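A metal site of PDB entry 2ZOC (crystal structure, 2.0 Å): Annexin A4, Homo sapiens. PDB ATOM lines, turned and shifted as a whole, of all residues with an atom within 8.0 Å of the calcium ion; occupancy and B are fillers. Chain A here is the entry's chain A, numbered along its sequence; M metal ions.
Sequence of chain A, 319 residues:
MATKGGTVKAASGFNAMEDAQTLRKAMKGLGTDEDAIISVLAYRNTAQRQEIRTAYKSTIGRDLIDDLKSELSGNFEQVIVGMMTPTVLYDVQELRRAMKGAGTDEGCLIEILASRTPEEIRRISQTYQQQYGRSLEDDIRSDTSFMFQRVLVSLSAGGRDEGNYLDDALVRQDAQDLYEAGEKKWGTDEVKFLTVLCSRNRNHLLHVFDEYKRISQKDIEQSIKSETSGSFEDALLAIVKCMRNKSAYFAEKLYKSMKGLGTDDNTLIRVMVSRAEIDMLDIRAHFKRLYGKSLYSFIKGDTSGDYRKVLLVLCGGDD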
ATOM      1  N   GLU A 221     -12.076  -1.029  14.967  1.00  0.00           N
ATOM      2  CA  GLU A 221     -11.922  -2.235  14.164  1.00  0.00           C
ATOM      3  C   GLU A 221     -13.007  -3.255  14.518  1.00  0.00           C
ATOM      4  O   GLU A 221     -13.518  -3.958  13.654  1.00  0.00           O
ATOM      5  CB  GLU A 221     -10.536  -2.880  14.372  1.00  0.00           C
ATOM      6  CG  GLU A 221      -9.379  -2.067  13.817  1.00  0.00           C
ATOM      7  CD  GLU A 221      -8.811  -1.084  14.825  1.00  0.00           C
ATOM      8  OE1 GLU A 221      -9.590  -0.513  15.610  1.00  0.00           O
ATOM      9  OE2 GLU A 221      -7.581  -0.878  14.816  1.00  0.00           O
ATOM     10  N   GLN A 222     -13.358  -3.331  15.802  1.00  0.00           N
ATOM     11  CA  GLN A 222     -14.390  -4.275  16.229  1.00  0.00           C
ATOM     12  C   GLN A 222     -15.754  -3.909  15.657  1.00  0.00           C
ATOM     13  O   GLN A 222     -16.505  -4.792  15.233  1.00  0.00           O
ATOM     14  CB  GLN A 222     -14.485  -4.318  17.754  1.00  0.00           C
ATOM     15  CG  GLN A 222     -13.160  -4.589  18.444  1.00  0.00           C
ATOM     16  CD  GLN A 222     -13.323  -4.808  19.934  1.00  0.00           C
ATOM     17  OE1 GLN A 222     -13.692  -5.901  20.372  1.00  0.00           O
ATOM     18  NE2 GLN A 222     -13.049  -3.777  20.718  1.00  0.00           N
ATOM     19  N   SER A 223     -16.059  -2.612  15.637  1.00  0.00           N
ATOM     20  CA  SER A 223     -17.344  -2.158  15.106  1.00  0.00           C
ATOM     21  C   SER A 223     -17.390  -2.311  13.591  1.00  0.00           C
ATOM     22  O   SER A 223     -18.413  -2.729  13.042  1.00  0.00           O
ATOM     23  CB  SER A 223     -17.592  -0.695  15.501  1.00  0.00           C
ATOM     24  OG  SER A 223     -17.927  -0.605  16.878  1.00  0.00           O
ATOM     25  N   ILE A 224     -16.295  -1.973  12.931  1.00  0.00           N
ATOM     26  CA  ILE A 224     -16.225  -2.114  11.478  1.00  0.00           C
ATOM     27  C   ILE A 224     -16.495  -3.573  11.108  1.00  0.00           C
ATOM     28  O   ILE A 224     -17.301  -3.858  10.234  1.00  0.00           O
ATOM     29  CB  ILE A 224     -14.832  -1.693  10.931  1.00  0.00           C
ATOM     30  CG1 ILE A 224     -14.718  -0.166  10.942  1.00  0.00           C
ATOM     31  CG2 ILE A 224     -14.621  -2.232   9.530  1.00  0.00           C
ATOM     32  CD1 ILE A 224     -13.331   0.324  10.693  1.00  0.00           C
ATOM     33  N   LYS A 225     -15.823  -4.494  11.798  1.00  0.00           N
ATOM     34  CA  LYS A 225     -16.006  -5.913  11.534  1.00  0.00           C
ATOM     35  C   LYS A 225     -17.441  -6.384  11.789  1.00  0.00           C
ATOM     36  O   LYS A 225     -17.985  -7.159  11.003  1.00  0.00           O
ATOM     37  CB  LYS A 225     -15.039  -6.753  12.383  1.00  0.00           C
ATOM     38  CG  LYS A 225     -13.576  -6.555  12.001  1.00  0.00           C
ATOM     39  CD  LYS A 225     -12.634  -7.375  12.865  1.00  0.00           C
ATOM     40  CE  LYS A 225     -11.193  -7.145  12.457  1.00  0.00           C
ATOM     41  NZ  LYS A 225     -10.233  -7.605  13.483  1.00  0.00           N
ATOM     42  N   SER A 226     -18.050  -5.908  12.868  1.00  0.00           N
ATOM     43  CA  SER A 226     -19.416  -6.323  13.182  1.00  0.00           C
ATOM     44  C   SER A 226     -20.478  -5.577  12.372  1.00  0.00           C
ATOM     45  O   SER A 226     -21.581  -6.089  12.151  1.00  0.00           O
ATOM     46  CB  SER A 226     -19.699  -6.163  14.687  1.00  0.00           C
ATOM     47  OG  SER A 226     -19.666  -4.810  15.108  1.00  0.00           O
ATOM     48  N   GLU A 227     -20.147  -4.383  11.893  1.00  0.00           N
ATOM     49  CA  GLU A 227     -21.108  -3.591  11.107  1.00  0.00           C
ATOM     50  C   GLU A 227     -21.046  -3.792   9.596  1.00  0.00           C
ATOM     51  O   GLU A 227     -22.060  -3.697   8.914  1.00  0.00           O
ATOM     52  CB  GLU A 227     -20.928  -2.106  11.422  1.00  0.00           C
ATOM     53  CG  GLU A 227     -21.350  -1.719  12.822  1.00  0.00           C
ATOM     54  CD  GLU A 227     -22.853  -1.692  12.980  1.00  0.00           C
ATOM     55  OE1 GLU A 227     -23.354  -2.005  14.099  1.00  0.00           O
ATOM     56  OE2 GLU A 227     -23.550  -1.337  11.998  1.00  0.00           O
ATOM     57  N   THR A 228     -19.857  -4.069   9.067  1.00  0.00           N
ATOM     58  CA  THR A 228     -19.697  -4.249   7.625  1.00  0.00           C
ATOM     59  C   THR A 228     -19.216  -5.649   7.236  1.00  0.00           C
ATOM     60  O   THR A 228     -18.995  -6.499   8.099  1.00  0.00           O
ATOM     61  CB  THR A 228     -18.695  -3.233   7.058  1.00  0.00           C
ATOM     62  OG1 THR A 228     -17.416  -3.419   7.676  1.00  0.00           O
ATOM     63  CG2 THR A 228     -19.189  -1.803   7.315  1.00  0.00           C
ATOM     64  N   SER A 229     -19.066  -5.878   5.930  1.00  0.00           N
ATOM     65  CA  SER A 229     -18.602  -7.164   5.447  1.00  0.00           C
ATOM     66  C   SER A 229     -18.037  -7.049   4.030  1.00  0.00           C
ATOM     67  O   SER A 229     -18.141  -6.001   3.395  1.00  0.00           O
ATOM     68  CB  SER A 229     -19.746  -8.186   5.448  1.00  0.00           C
ATOM     69  OG  SER A 229     -20.828  -7.744   4.650  1.00  0.00           O
ATOM     70  N   GLY A 230     -17.425  -8.113   3.550  1.00  0.00           N
ATOM     71  CA  GLY A 230     -16.876  -8.112   2.220  1.00  0.00           C
ATOM     72  C   GLY A 230     -15.778  -7.089   1.982  1.00  0.00           C
ATOM     73  O   GLY A 230     -15.143  -6.606   2.923  1.00  0.00           O
ATOM     74  N   GLU A 233     -15.622  -3.833   3.982  1.00  0.00           N
ATOM     75  CA  GLU A 233     -15.006  -4.031   5.299  1.00  0.00           C
ATOM     76  C   GLU A 233     -13.489  -4.047   5.157  1.00  0.00           C
ATOM     77  O   GLU A 233     -12.769  -3.381   5.902  1.00  0.00           O
ATOM     78  CB  GLU A 233     -15.469  -5.364   5.913  1.00  0.00           C
ATOM     79  CG  GLU A 233     -14.964  -5.629   7.333  1.00  0.00           C
ATOM     80  CD  GLU A 233     -15.338  -7.009   7.850  1.00  0.00           C
ATOM     81  OE1 GLU A 233     -16.479  -7.453   7.604  1.00  0.00           O
ATOM     82  OE2 GLU A 233     -14.493  -7.665   8.497  1.00  0.00           O
ATOM     83  N   ASP A 234     -12.991  -4.803   4.185  1.00  0.00           N
ATOM     84  CA  ASP A 234     -11.563  -4.912   3.954  1.00  0.00           C
ATOM     85  C   ASP A 234     -10.925  -3.542   3.688  1.00  0.00           C
ATOM     86  O   ASP A 234      -9.848  -3.237   4.210  1.00  0.00           O
ATOM     87  CB  ASP A 234     -11.259  -5.863   2.779  1.00  0.00           C
ATOM     88  CG  ASP A 234     -11.730  -7.288   3.038  1.00  0.00           C
ATOM     89  OD1 ASP A 234     -11.773  -7.715   4.204  1.00  0.00           O
ATOM     90  OD2 ASP A 234     -12.049  -7.990   2.055  1.00  0.00           O
ATOM     91  N   LEU A 237     -10.889  -1.519   6.955  1.00  0.00           N
ATOM     92  CA  LEU A 237      -9.882  -2.020   7.869  1.00  0.00           C
ATOM     93  C   LEU A 237      -8.464  -1.651   7.428  1.00  0.00           C
ATOM     94  O   LEU A 237      -7.602  -1.343   8.260  1.00  0.00           O
ATOM     95  CB  LEU A 237      -9.998  -3.548   8.008  1.00  0.00           C
ATOM     96  CG  LEU A 237     -11.278  -4.082   8.672  1.00  0.00           C
ATOM     97  CD1 LEU A 237     -11.221  -5.601   8.748  1.00  0.00           C
ATOM     98  CD2 LEU A 237     -11.425  -3.492  10.060  1.00  0.00           C
HETATM   99 CA    CA M   1     -18.050  -8.309   9.155  1.00  0.00          CA
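Ser 229 touches the calcium ion. Four residues have an atom within 4 Å of the calcium ion: Lys 225, Thr 228, Ser 229 and Glu 233.
The backbone carbonyl oxygen of Ile 224 lies within hydrogen-bond range of the side-chain hydroxyl of Thr 228 (2.6 Å). The side-chain carboxylate of Glu 233 lies close to the backbone NH of Ser 229 (3.5 Å).
The calcium ion is bound by the backbone carbonyl oxygen (O) of Lys 225 (2.2 Å). The calcium ion is bound by O of Thr 228, 2.3 Å away. OE1 of Glu 233 binds the calcium ion (2.4 Å). The calcium ion has three donor atoms within binding distance.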
